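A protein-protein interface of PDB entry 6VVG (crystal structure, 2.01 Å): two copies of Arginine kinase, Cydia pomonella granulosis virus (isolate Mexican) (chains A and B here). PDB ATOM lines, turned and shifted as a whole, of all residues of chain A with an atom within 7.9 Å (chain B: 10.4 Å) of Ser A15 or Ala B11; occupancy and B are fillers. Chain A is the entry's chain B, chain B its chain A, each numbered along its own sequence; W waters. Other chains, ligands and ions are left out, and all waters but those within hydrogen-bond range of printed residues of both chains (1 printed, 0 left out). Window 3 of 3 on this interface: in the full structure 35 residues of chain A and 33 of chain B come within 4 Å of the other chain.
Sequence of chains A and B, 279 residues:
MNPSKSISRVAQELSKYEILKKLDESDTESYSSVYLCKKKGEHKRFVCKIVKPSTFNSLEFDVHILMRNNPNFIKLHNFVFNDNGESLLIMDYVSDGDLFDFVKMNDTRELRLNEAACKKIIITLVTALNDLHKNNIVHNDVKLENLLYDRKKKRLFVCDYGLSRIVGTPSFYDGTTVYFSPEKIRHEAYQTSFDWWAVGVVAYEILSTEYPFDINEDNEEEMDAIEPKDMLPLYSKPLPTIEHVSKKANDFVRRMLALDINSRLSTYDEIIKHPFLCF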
ATOM      1  N   ILE A   7       7.789   2.026  16.255  1.00  0.00           N
ATOM      2  CA  ILE A   7       8.099   1.053  15.210  1.00  0.00           C
ATOM      3  C   ILE A   7       8.118  -0.352  15.795  1.00  0.00           C
ATOM      4  O   ILE A   7       7.520  -1.284  15.244  1.00  0.00           O
ATOM      5  CB  ILE A   7       9.436   1.399  14.529  1.00  0.00           C
ATOM      6  CG1 ILE A   7       9.408   2.840  14.016  1.00  0.00           C
ATOM      7  CG2 ILE A   7       9.708   0.424  13.403  1.00  0.00           C
ATOM      8  CD1 ILE A   7      10.314   3.105  12.837  1.00  0.00           C
ATOM      9  N   SER A   8       8.819  -0.525  16.917  1.00  0.00           N
ATOM     10  CA  SER A   8       8.849  -1.823  17.581  1.00  0.00           C
ATOM     11  C   SER A   8       7.439  -2.327  17.857  1.00  0.00           C
ATOM     12  O   SER A   8       7.103  -3.471  17.532  1.00  0.00           O
ATOM     13  CB  SER A   8       9.647  -1.726  18.882  1.00  0.00           C
ATOM     14  OG  SER A   8      11.002  -1.403  18.629  1.00  0.00           O
ATOM     15  N   ARG A   9       6.595  -1.479  18.455  1.00  0.00           N
ATOM     16  CA  ARG A   9       5.234  -1.896  18.774  1.00  0.00           C
ATOM     17  C   ARG A   9       4.452  -2.223  17.507  1.00  0.00           C
ATOM     18  O   ARG A   9       3.718  -3.219  17.463  1.00  0.00           O
ATOM     19  CB  ARG A   9       4.526  -0.799  19.581  1.00  0.00           C
ATOM     20  N   VAL A  10       4.582  -1.382  16.475  1.00  0.00           N
ATOM     21  CA  VAL A  10       3.847  -1.609  15.235  1.00  0.00           C
ATOM     22  C   VAL A  10       4.247  -2.948  14.630  1.00  0.00           C
ATOM     23  O   VAL A  10       3.394  -3.748  14.234  1.00  0.00           O
ATOM     24  CB  VAL A  10       4.069  -0.444  14.252  1.00  0.00           C
ATOM     25  CG1 VAL A  10       3.908  -0.922  12.820  1.00  0.00           C
ATOM     26  CG2 VAL A  10       3.094   0.692  14.568  1.00  0.00           C
ATOM     27  N   ALA A  11       5.553  -3.214  14.551  1.00  0.00           N
ATOM     28  CA  ALA A  11       6.006  -4.522  14.082  1.00  0.00           C
ATOM     29  C   ALA A  11       5.483  -5.638  14.980  1.00  0.00           C
ATOM     30  O   ALA A  11       5.062  -6.693  14.494  1.00  0.00           O
ATOM     31  CB  ALA A  11       7.533  -4.554  14.018  1.00  0.00           C
ATOM     32  N   GLN A  12       5.491  -5.413  16.295  1.00  0.00           N
ATOM     33  CA  GLN A  12       5.066  -6.440  17.242  1.00  0.00           C
ATOM     34  C   GLN A  12       3.610  -6.833  17.018  1.00  0.00           C
ATOM     35  O   GLN A  12       3.278  -8.022  16.965  1.00  0.00           O
ATOM     36  CB  GLN A  12       5.272  -5.928  18.668  1.00  0.00           C
ATOM     37  CG  GLN A  12       5.678  -6.971  19.685  1.00  0.00           C
ATOM     38  CD  GLN A  12       5.823  -6.379  21.081  1.00  0.00           C
ATOM     39  OE1 GLN A  12       5.126  -6.781  22.012  1.00  0.00           O
ATOM     40  NE2 GLN A  12       6.723  -5.412  21.227  1.00  0.00           N
ATOM     41  N   GLU A  13       2.725  -5.841  16.894  1.00  0.00           N
ATOM     42  CA  GLU A  13       1.307  -6.125  16.704  1.00  0.00           C
ATOM     43  C   GLU A  13       1.089  -7.061  15.520  1.00  0.00           C
ATOM     44  O   GLU A  13       0.333  -8.034  15.609  1.00  0.00           O
ATOM     45  CB  GLU A  13       0.547  -4.812  16.509  1.00  0.00           C
ATOM     46  CG  GLU A  13      -0.849  -4.951  15.926  1.00  0.00           C
ATOM     47  CD  GLU A  13      -1.870  -5.450  16.933  1.00  0.00           C
ATOM     48  OE1 GLU A  13      -1.458  -5.904  18.021  1.00  0.00           O
ATOM     49  OE2 GLU A  13      -3.085  -5.385  16.642  1.00  0.00           O
ATOM     50  N   LEU A  14       1.738  -6.770  14.395  1.00  0.00           N
ATOM     51  CA  LEU A  14       1.546  -7.581  13.200  1.00  0.00           C
ATOM     52  C   LEU A  14       2.174  -8.962  13.320  1.00  0.00           C
ATOM     53  O   LEU A  14       1.726  -9.894  12.647  1.00  0.00           O
ATOM     54  CB  LEU A  14       2.124  -6.871  11.989  1.00  0.00           C
ATOM     55  CG  LEU A  14       1.341  -5.638  11.560  1.00  0.00           C
ATOM     56  CD1 LEU A  14       2.272  -4.470  11.249  1.00  0.00           C
ATOM     57  CD2 LEU A  14       0.467  -5.987  10.361  1.00  0.00           C
ATOM     58  N   SER A  15       3.171  -9.121  14.190  1.00  0.00           N
ATOM     59  CA  SER A  15       3.822 -10.406  14.387  1.00  0.00           C
ATOM     60  C   SER A  15       2.940 -11.408  15.114  1.00  0.00           C
ATOM     61  O   SER A  15       3.262 -12.599  15.111  1.00  0.00           O
ATOM     62  CB  SER A  15       5.122 -10.194  15.163  1.00  0.00           C
ATOM     63  OG  SER A  15       6.031  -9.399  14.417  1.00  0.00           O
ATOM     64  N   LYS A  16       1.831 -10.960  15.703  1.00  0.00           N
ATOM     65  CA  LYS A  16       0.964 -11.862  16.448  1.00  0.00           C
ATOM     66  C   LYS A  16       0.131 -12.757  15.540  1.00  0.00           C
ATOM     67  O   LYS A  16      -0.425 -13.750  16.018  1.00  0.00           O
ATOM     68  CB  LYS A  16       0.049 -11.052  17.367  1.00  0.00           C
ATOM     69  CG  LYS A  16       0.771 -10.397  18.537  1.00  0.00           C
ATOM     70  CD  LYS A  16      -0.076  -9.325  19.212  1.00  0.00           C
ATOM     71  CE  LYS A  16       0.371  -9.116  20.655  1.00  0.00           C
ATOM     72  NZ  LYS A  16       0.170  -7.716  21.121  1.00  0.00           N
ATOM     73  N   TYR A  17       0.043 -12.442  14.251  1.00  0.00           N
ATOM     74  CA  TYR A  17      -0.782 -13.208  13.327  1.00  0.00           C
ATOM     75  C   TYR A  17       0.004 -14.378  12.748  1.00  0.00           C
ATOM     76  O   TYR A  17       1.197 -14.258  12.454  1.00  0.00           O
ATOM     77  CB  TYR A  17      -1.288 -12.320  12.190  1.00  0.00           C
ATOM     78  CG  TYR A  17      -2.250 -11.232  12.615  1.00  0.00           C
ATOM     79  CD1 TYR A  17      -3.593 -11.508  12.817  1.00  0.00           C
ATOM     80  CD2 TYR A  17      -1.814  -9.927  12.804  1.00  0.00           C
ATOM     81  CE1 TYR A  17      -4.477 -10.519  13.201  1.00  0.00           C
ATOM     82  CE2 TYR A  17      -2.690  -8.929  13.191  1.00  0.00           C
ATOM     83  CZ  TYR A  17      -4.022  -9.232  13.387  1.00  0.00           C
ATOM     84  OH  TYR A  17      -4.902  -8.247  13.772  1.00  0.00           O
ATOM     85  N   GLU A  18      -0.682 -15.510  12.577  1.00  0.00           N
ATOM     86  CA  GLU A  18      -0.103 -16.703  11.972  1.00  0.00           C
ATOM     87  C   GLU A  18      -1.054 -17.273  10.928  1.00  0.00           C
ATOM     88  O   GLU A  18      -2.263 -17.390  11.158  1.00  0.00           O
ATOM     89  CB  GLU A  18       0.227 -17.780  13.029  1.00  0.00           C
ATOM     90  CG  GLU A  18      -0.772 -17.903  14.162  1.00  0.00           C
ATOM     91  CD  GLU A  18      -0.165 -18.537  15.411  1.00  0.00           C
ATOM     92  OE1 GLU A  18       1.074 -18.709  15.457  1.00  0.00           O
ATOM     93  OE2 GLU A  18      -0.923 -18.871  16.347  1.00  0.00           O
ATOM     94  N   LYS A  38      -4.868 -16.772  12.281  1.00  0.00           N
ATOM     95  CA  LYS A  38      -5.201 -16.741  13.695  1.00  0.00           C
ATOM     96  C   LYS A  38      -4.215 -15.830  14.416  1.00  0.00           C
ATOM     97  O   LYS A  38      -3.069 -15.668  13.989  1.00  0.00           O
ATOM     98  CB  LYS A  38      -5.171 -18.143  14.315  1.00  0.00           C
ATOM     99  CG  LYS A  38      -5.417 -18.147  15.815  1.00  0.00           C
ATOM    100  CD  LYS A  38      -6.280 -19.338  16.256  1.00  0.00           C
ATOM    101  CE  LYS A  38      -6.316 -19.481  17.781  1.00  0.00           C
ATOM    102  NZ  LYS A  38      -5.222 -18.734  18.480  1.00  0.00           N
ATOM    103  N   LYS A  39      -4.684 -15.219  15.498  1.00  0.00           N
ATOM    104  CA  LYS A  39      -3.913 -14.278  16.294  1.00  0.00           C
ATOM    105  C   LYS A  39      -3.582 -14.926  17.627  1.00  0.00           C
ATOM    106  O   LYS A  39      -4.420 -15.631  18.200  1.00  0.00           O
ATOM    107  CB  LYS A  39      -4.706 -12.991  16.518  1.00  0.00           C
ATOM    108  CG  LYS A  39      -3.894 -11.795  16.950  1.00  0.00           C
ATOM    109  CD  LYS A  39      -4.683 -10.521  16.672  1.00  0.00           C
ATOM    110  CE  LYS A  39      -3.825  -9.283  16.850  1.00  0.00           C
ATOM    111  NZ  LYS A  39      -4.163  -8.559  18.111  1.00  0.00           N
ATOM    112  N   LYS A  40      -2.356 -14.707  18.110  1.00  0.00           N
ATOM    113  CA  LYS A  40      -1.935 -15.295  19.385  1.00  0.00           C
ATOM    114  C   LYS A  40      -2.778 -14.717  20.525  1.00  0.00           C
ATOM    115  O   LYS A  40      -2.813 -13.500  20.725  1.00  0.00           O
ATOM    116  CB  LYS A  40      -0.439 -15.031  19.624  1.00  0.00           C
ATOM    117  N   ASN A  78      -5.538  -4.491  10.164  1.00  0.00           N
ATOM    118  CA  ASN A  78      -4.203  -4.033   9.811  1.00  0.00           C
ATOM    119  C   ASN A  78      -4.084  -3.957   8.296  1.00  0.00           C
ATOM    120  O   ASN A  78      -4.763  -4.682   7.565  1.00  0.00           O
ATOM    121  CB  ASN A  78      -3.112  -4.958  10.377  1.00  0.00           C
ATOM    122  CG  ASN A  78      -3.437  -5.469  11.769  1.00  0.00           C
ATOM    123  OD1 ASN A  78      -4.238  -6.390  11.935  1.00  0.00           O
ATOM    124  ND2 ASN A  78      -2.816  -4.874  12.779  1.00  0.00           N
ATOM    125  N   VAL A  80      -0.693  -3.284   5.518  1.00  0.00           N
ATOM    126  CA  VAL A  80       0.726  -3.037   5.297  1.00  0.00           C
ATOM    127  C   VAL A  80       0.928  -2.806   3.808  1.00  0.00           C
ATOM    128  O   VAL A  80       0.567  -3.661   2.988  1.00  0.00           O
ATOM    129  CB  VAL A  80       1.598  -4.203   5.791  1.00  0.00           C
ATOM    130  CG1 VAL A  80       3.076  -3.863   5.631  1.00  0.00           C
ATOM    131  CG2 VAL A  80       1.272  -4.540   7.237  1.00  0.00           C
ATOM    132  N   ASN A  82       3.845  -1.805   0.836  1.00  0.00           N
ATOM    133  CA  ASN A  82       5.260  -1.754   0.484  1.00  0.00           C
ATOM    134  C   ASN A  82       5.358  -1.377  -0.987  1.00  0.00           C
ATOM    135  O   ASN A  82       4.891  -2.129  -1.848  1.00  0.00           O
ATOM    136  CB  ASN A  82       5.942  -3.103   0.735  1.00  0.00           C
ATOM    137  CG  ASN A  82       6.430  -3.252   2.159  1.00  0.00           C
ATOM    138  OD1 ASN A  82       5.637  -3.300   3.098  1.00  0.00           O
ATOM    139  ND2 ASN A  82       7.745  -3.328   2.328  1.00  0.00           N
ATOM    140  N   ILE A  90      -5.418  -7.439   6.699  1.00  0.00           N
ATOM    141  CA  ILE A  90      -5.869  -8.373   7.727  1.00  0.00           C
ATOM    142  C   ILE A  90      -7.240  -7.911   8.199  1.00  0.00           C
ATOM    143  O   ILE A  90      -7.375  -6.819   8.765  1.00  0.00           O
ATOM    144  CB  ILE A  90      -4.877  -8.457   8.897  1.00  0.00           C
ATOM    145  CG1 ILE A  90      -3.544  -9.026   8.406  1.00  0.00           C
ATOM    146  CG2 ILE A  90      -5.444  -9.315  10.017  1.00  0.00           C
ATOM    147  CD1 ILE A  90      -2.465  -9.108   9.465  1.00  0.00           C
ATOM    148  N   SER B   4       3.365 -16.519   4.912  1.00  0.00           N
ATOM    149  CA  SER B   4       3.736 -16.311   6.305  1.00  0.00           C
ATOM    150  C   SER B   4       5.161 -15.776   6.451  1.00  0.00           C
ATOM    151  O   SER B   4       5.535 -15.378   7.553  1.00  0.00           O
ATOM    152  CB  SER B   4       3.600 -17.584   7.165  1.00  0.00           C
ATOM    153  OG  SER B   4       3.976 -17.328   8.510  1.00  0.00           O
ATOM    154  N   LYS B   5       5.961 -15.729   5.383  1.00  0.00           N
ATOM    155  CA  LYS B   5       7.210 -14.980   5.434  1.00  0.00           C
ATOM    156  C   LYS B   5       6.954 -13.504   5.167  1.00  0.00           C
ATOM    157  O   LYS B   5       7.736 -12.649   5.600  1.00  0.00           O
ATOM    158  CB  LYS B   5       8.212 -15.547   4.420  1.00  0.00           C
ATOM    159  N   SER B   6       5.873 -13.195   4.445  1.00  0.00           N
ATOM    160  CA  SER B   6       5.495 -11.803   4.222  1.00  0.00           C
ATOM    161  C   SER B   6       5.338 -11.069   5.545  1.00  0.00           C
ATOM    162  O   SER B   6       5.909  -9.989   5.744  1.00  0.00           O
ATOM    163  CB  SER B   6       4.198 -11.738   3.410  1.00  0.00           C
ATOM    164  N   ILE B   7       4.563 -11.642   6.469  1.00  0.00           N
ATOM    165  CA  ILE B   7       4.323 -10.989   7.755  1.00  0.00           C
ATOM    166  C   ILE B   7       5.642 -10.645   8.429  1.00  0.00           C
ATOM    167  O   ILE B   7       5.892  -9.495   8.809  1.00  0.00           O
ATOM    168  CB  ILE B   7       3.461 -11.884   8.662  1.00  0.00           C
ATOM    169  CG1 ILE B   7       1.985 -11.765   8.289  1.00  0.00           C
ATOM    170  CG2 ILE B   7       3.666 -11.510  10.124  1.00  0.00           C
ATOM    171  CD1 ILE B   7       1.217 -13.066   8.425  1.00  0.00           C
ATOM    172  N   SER B   8       6.500 -11.651   8.613  1.00  0.00           N
ATOM    173  CA  SER B   8       7.761 -11.408   9.301  1.00  0.00           C
ATOM    174  C   SER B   8       8.709 -10.547   8.472  1.00  0.00           C
ATOM    175  O   SER B   8       9.567  -9.870   9.049  1.00  0.00           O
ATOM    176  CB  SER B   8       8.421 -12.734   9.677  1.00  0.00           C
ATOM    177  OG  SER B   8       7.806 -13.276  10.834  1.00  0.00           O
ATOM    178  N   ARG B   9       8.582 -10.550   7.138  1.00  0.00           N
ATOM    179  CA  ARG B   9       9.370  -9.634   6.325  1.00  0.00           C
ATOM    180  C   ARG B   9       8.939  -8.187   6.575  1.00  0.00           C
ATOM    181  O   ARG B   9       9.763  -7.277   6.604  1.00  0.00           O
ATOM    182  CB  ARG B   9       9.235 -10.019   4.837  1.00  0.00           C
ATOM    183  N   VAL B  10       7.634  -7.975   6.703  1.00  0.00           N
ATOM    184  CA  VAL B  10       7.135  -6.663   7.095  1.00  0.00           C
ATOM    185  C   VAL B  10       7.767  -6.225   8.408  1.00  0.00           C
ATOM    186  O   VAL B  10       8.293  -5.108   8.525  1.00  0.00           O
ATOM    187  CB  VAL B  10       5.609  -6.699   7.233  1.00  0.00           C
ATOM    188  CG1 VAL B  10       5.192  -5.415   8.052  1.00  0.00           C
ATOM    189  CG2 VAL B  10       4.907  -6.834   5.978  1.00  0.00           C
ATOM    190  N   ALA B  11       7.792  -7.111   9.394  1.00  0.00           N
ATOM    191  CA  ALA B  11       8.440  -6.811  10.667  1.00  0.00           C
ATOM    192  C   ALA B  11       9.947  -6.659  10.504  1.00  0.00           C
ATOM    193  O   ALA B  11      10.591  -5.849  11.192  1.00  0.00           O
ATOM    194  CB  ALA B  11       8.111  -7.932  11.643  1.00  0.00           C
ATOM    195  N   GLN B  12      10.525  -7.429   9.589  1.00  0.00           N
ATOM    196  CA  GLN B  12      11.953  -7.322   9.338  1.00  0.00           C
ATOM    197  C   GLN B  12      12.285  -6.019   8.621  1.00  0.00           C
ATOM    198  O   GLN B  12      13.193  -5.290   9.040  1.00  0.00           O
ATOM    199  CB  GLN B  12      12.445  -8.524   8.531  1.00  0.00           C
ATOM    200  N   GLU B  13      11.572  -5.712   7.530  1.00  0.00           N
ATOM    201  CA  GLU B  13      11.855  -4.494   6.782  1.00  0.00           C
ATOM    202  C   GLU B  13      11.661  -3.264   7.665  1.00  0.00           C
ATOM    203  O   GLU B  13      12.573  -2.446   7.828  1.00  0.00           O
ATOM    204  CB  GLU B  13      10.957  -4.414   5.537  1.00  0.00           C
ATOM    205  CG  GLU B  13      11.236  -3.184   4.679  1.00  0.00           C
ATOM    206  CD  GLU B  13      12.726  -2.910   4.497  1.00  0.00           C
ATOM    207  OE1 GLU B  13      13.432  -3.782   3.944  1.00  0.00           O
ATOM    208  OE2 GLU B  13      13.194  -1.829   4.917  1.00  0.00           O
ATOM    209  N   LEU B  14      10.455  -3.110   8.222  1.00  0.00           N
ATOM    210  CA  LEU B  14      10.142  -1.931   9.017  1.00  0.00           C
ATOM    211  C   LEU B  14      10.853  -1.920  10.364  1.00  0.00           C
ATOM    212  O   LEU B  14      10.654  -0.974  11.137  1.00  0.00           O
ATOM    213  CB  LEU B  14       8.633  -1.830   9.225  1.00  0.00           C
ATOM    214  CG  LEU B  14       8.030  -0.520   9.731  1.00  0.00           C
ATOM    215  CD1 LEU B  14       7.504   0.327   8.611  1.00  0.00           C
ATOM    216  CD2 LEU B  14       6.905  -0.877  10.713  1.00  0.00           C
ATOM    217  N   SER B  15      11.679  -2.921  10.660  1.00  0.00           N
ATOM    218  CA  SER B  15      12.553  -2.899  11.826  1.00  0.00           C
ATOM    219  C   SER B  15      13.924  -2.313  11.520  1.00  0.00           C
ATOM    220  O   SER B  15      14.742  -2.168  12.436  1.00  0.00           O
ATOM    221  CB  SER B  15      12.723  -4.316  12.384  1.00  0.00           C
ATOM    222  OG  SER B  15      13.880  -4.412  13.202  1.00  0.00           O
ATOM    223  N   LYS B  16      14.197  -1.986  10.258  1.00  0.00           N
ATOM    224  CA  LYS B  16      15.477  -1.397   9.890  1.00  0.00           C
ATOM    225  C   LYS B  16      15.531   0.101  10.160  1.00  0.00           C
ATOM    226  O   LYS B  16      16.628   0.669  10.221  1.00  0.00           O
ATOM    227  CB  LYS B  16      15.761  -1.651   8.408  1.00  0.00           C
ATOM    228  CG  LYS B  16      15.903  -3.112   8.020  1.00  0.00           C
ATOM    229  CD  LYS B  16      16.311  -3.238   6.552  1.00  0.00           C
ATOM    230  CE  LYS B  16      16.228  -4.675   6.062  1.00  0.00           C
ATOM    231  NZ  LYS B  16      15.413  -4.786   4.817  1.00  0.00           N
ATOM    232  N   TYR B  17      14.381   0.748  10.325  1.00  0.00           N
ATOM    233  CA  TYR B  17      14.330   2.198  10.442  1.00  0.00           C
ATOM    234  C   TYR B  17      14.653   2.649  11.861  1.00  0.00           C
ATOM    235  O   TYR B  17      14.178   2.068  12.840  1.00  0.00           O
ATOM    236  CB  TYR B  17      12.948   2.700  10.028  1.00  0.00           C
ATOM    237  CG  TYR B  17      12.733   2.693   8.532  1.00  0.00           C
ATOM    238  CD1 TYR B  17      13.201   3.732   7.743  1.00  0.00           C
ATOM    239  CD2 TYR B  17      12.069   1.644   7.907  1.00  0.00           C
ATOM    240  CE1 TYR B  17      13.013   3.734   6.377  1.00  0.00           C
ATOM    241  CE2 TYR B  17      11.874   1.638   6.538  1.00  0.00           C
ATOM    242  CZ  TYR B  17      12.350   2.684   5.779  1.00  0.00           C
ATOM    243  OH  TYR B  17      12.160   2.685   4.416  1.00  0.00           O
ATOM    244  N   ASN B  78       6.594   3.032   2.698  1.00  0.00           N
ATOM    245  CA  ASN B  78       5.949   2.026   3.527  1.00  0.00           C
ATOM    246  C   ASN B  78       4.797   2.669   4.282  1.00  0.00           C
ATOM    247  O   ASN B  78       4.798   3.877   4.524  1.00  0.00           O
ATOM    248  CB  ASN B  78       6.928   1.393   4.520  1.00  0.00           C
ATOM    249  CG  ASN B  78       8.150   0.813   3.844  1.00  0.00           C
ATOM    250  OD1 ASN B  78       8.198  -0.380   3.545  1.00  0.00           O
ATOM    251  ND2 ASN B  78       9.145   1.655   3.596  1.00  0.00           N
ATOM    252  N   PHE B  79       3.817   1.848   4.657  1.00  0.00           N
ATOM    253  CA  PHE B  79       2.651   2.324   5.387  1.00  0.00           C
ATOM    254  C   PHE B  79       2.059   1.142   6.137  1.00  0.00           C
ATOM    255  O   PHE B  79       1.783   0.098   5.539  1.00  0.00           O
ATOM    256  CB  PHE B  79       1.628   2.957   4.436  1.00  0.00           C
ATOM    257  CG  PHE B  79       0.299   3.240   5.070  1.00  0.00           C
ATOM    258  CD1 PHE B  79       0.200   4.014   6.219  1.00  0.00           C
ATOM    259  CD2 PHE B  79      -0.859   2.737   4.506  1.00  0.00           C
ATOM    260  CE1 PHE B  79      -1.037   4.267   6.792  1.00  0.00           C
ATOM    261  CE2 PHE B  79      -2.090   2.987   5.069  1.00  0.00           C
ATOM    262  CZ  PHE B  79      -2.184   3.752   6.213  1.00  0.00           C
ATOM    263  N   VAL B  80       1.895   1.306   7.445  1.00  0.00           N
ATOM    264  CA  VAL B  80       1.323   0.287   8.311  1.00  0.00           C
ATOM    265  C   VAL B  80       0.177   0.942   9.067  1.00  0.00           C
ATOM    266  O   VAL B  80       0.404   1.856   9.869  1.00  0.00           O
ATOM    267  CB  VAL B  80       2.355  -0.295   9.285  1.00  0.00           C
ATOM    268  CG1 VAL B  80       1.691  -1.339  10.165  1.00  0.00           C
ATOM    269  CG2 VAL B  80       3.534  -0.878   8.530  1.00  0.00           C
ATOM    270  N   ASN B  82      -2.907   0.348  11.788  1.00  0.00           N
ATOM    271  CA  ASN B  82      -3.411  -0.519  12.849  1.00  0.00           C
ATOM    272  C   ASN B  82      -4.701   0.073  13.396  1.00  0.00           C
ATOM    273  O   ASN B  82      -4.738   1.251  13.764  1.00  0.00           O
ATOM    274  CB  ASN B  82      -2.391  -0.683  13.980  1.00  0.00           C
ATOM    275  CG  ASN B  82      -1.148  -1.410  13.536  1.00  0.00           C
ATOM    276  OD1 ASN B  82      -1.178  -2.609  13.251  1.00  0.00           O
ATOM    277  ND2 ASN B  82      -0.040  -0.686  13.470  1.00  0.00           N
ATOM    278  N   LEU B  88       1.890   4.066  10.676  1.00  0.00           N
ATOM    279  CA  LEU B  88       3.140   4.642  10.211  1.00  0.00           C
ATOM    280  C   LEU B  88       3.083   4.933   8.721  1.00  0.00           C
ATOM    281  O   LEU B  88       2.611   4.108   7.936  1.00  0.00           O
ATOM    282  CB  LEU B  88       4.303   3.686  10.468  1.00  0.00           C
ATOM    283  CG  LEU B  88       4.501   3.089  11.858  1.00  0.00           C
ATOM    284  CD1 LEU B  88       5.887   2.433  11.943  1.00  0.00           C
ATOM    285  CD2 LEU B  88       4.340   4.159  12.909  1.00  0.00           C
ATOM    286  N   ILE B  90       6.060   5.987   6.003  1.00  0.00           N
ATOM    287  CA  ILE B  90       7.474   6.240   5.737  1.00  0.00           C
ATOM    288  C   ILE B  90       7.582   6.779   4.318  1.00  0.00           C
ATOM    289  O   ILE B  90       7.298   6.064   3.348  1.00  0.00           O
ATOM    290  CB  ILE B  90       8.334   4.984   5.927  1.00  0.00           C
ATOM    291  CG1 ILE B  90       8.207   4.481   7.366  1.00  0.00           C
ATOM    292  CG2 ILE B  90       9.786   5.286   5.589  1.00  0.00           C
ATOM    293  CD1 ILE B  90       8.949   3.189   7.639  1.00  0.00           C
HETATM  294  O   HOH W   1       5.857  -1.579   5.174  1.00  0.00           O
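The side-chain amide oxygen (OD1) of Asn B82 lies within hydrogen-bond range of the side-chain amide nitrogen (ND2) of Asn A78 (2.8 Å). The side-chain amide nitrogen (ND2) of Asn A82 is in hydrogen-bond range of the side-chain amide oxygen (OD1) of Asn B78 (3.2 Å).
N of Ile B90 sits at hydrogen-bond distance from O of Asn B78 (2.9 Å). The side-chain amino group (NZ) of Lys A16 lies within salt-bridge range of the side-chain carboxylate (OE1) of Glu A13 (3.9 Å). The side-chain amide oxygen (OD1) of Asn A78 is in hydrogen-bond range of the side-chain hydroxyl (OH) of Tyr A17 (2.7 Å). The side-chain hydroxyl (OH) of Tyr B17 lies within hydrogen-bond range of the side-chain amide nitrogen (ND2) of Asn B78, 3.3 Å away. The backbone carbonyl oxygen (O) of Val B80 sits at hydrogen-bond distance from the backbone NH (N) of Leu B88 (2.8 Å). The backbone carbonyl oxygen of Ala A11 is in hydrogen-bond range of the side-chain hydroxyl of Ser A15 (2.9 Å).
Among the printed residues, pairs that only touch across the chains: Ile A7 with Leu B14, Ile A7 with Tyr B17, Val A10 with Leu B14, Val A10 with Val B80, Val A10 with Asn B82, Val A10 with Leu B88, Glu A13 with Asn B82, Leu A14 with Ile B7, Leu A14 with Val B80, Ser A15 with Ala B11, Val A80 with Val B10 and Val A80 with Phe B79.
No residue of chain B comes within 4 Å of Ala A11. Leu A14 touches just these residues of chain B: Ile B7 and Val B80. Of chain B, only Ala B11 comes within 4 Å of Ser A15. Printed residues of chain A within 4 Å of Ile B7: Leu A14 (3.6 Å). Printed residues of chain A within 4 Å of Val B10: Val A80 (3.5 Å). Ala B11 touches just one residue of chain A: Ser A15. No residue of chain A comes within 4 Å of Gln B12. The nearest residue of chain A that does not touch Ala B11 is Ala A11 (4.1 Å). The nearest printed residue of chain A that does not touch Leu B88 is Ile A7 (4.1 Å).
Hydrophobic or aromatic side chains of chain A within 4 Å of the printed part of chain B: Ile A7, Val A10, Leu A14 and Val A80. Of the 20 printed residues of chain B, 10 touch a printed residue of chain A. Hydrophobic or aromatic side chains of chain B within 4 Å of the printed part of chain A: Ile B7, Val B10, Ala B11, Leu B14, Tyr B17, Val B80 and Leu B88. Among the printed residues, 14 pairs touch across the chains. Among the printed residues, no Asp or Glu carboxylate lies within 4 Å of a Lys or Arg side-chain nitrogen of the other chain.
Val A10 touches Val B80, and with the chains exchanged Val A80 touches Val B10. Leu A14 touches Val B80, but with the chains exchanged Val A80 does not touch Leu B14 (6.8 Å). Ser A15 touches Ala B11, but with the chains exchanged Ala A11 does not touch Ser B15 (5.4 Å). Asn A78 touches Asn B82, and with the chains exchanged Asn A82 touches Asn B78. Positions printed for both chains: 7, 8, 9, 10, 11, 12, 13, 14, 15, 16, 17, 78, 80, 82 and 90. Of the 14 pairs that touch across the chains among the printed residues, 6 have their exchanged pair printed and touching as well.
Water W1 bridges OD1 of Asn A82 (2.7 Å) and OD1 of Asn B78 (3.1 Å).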
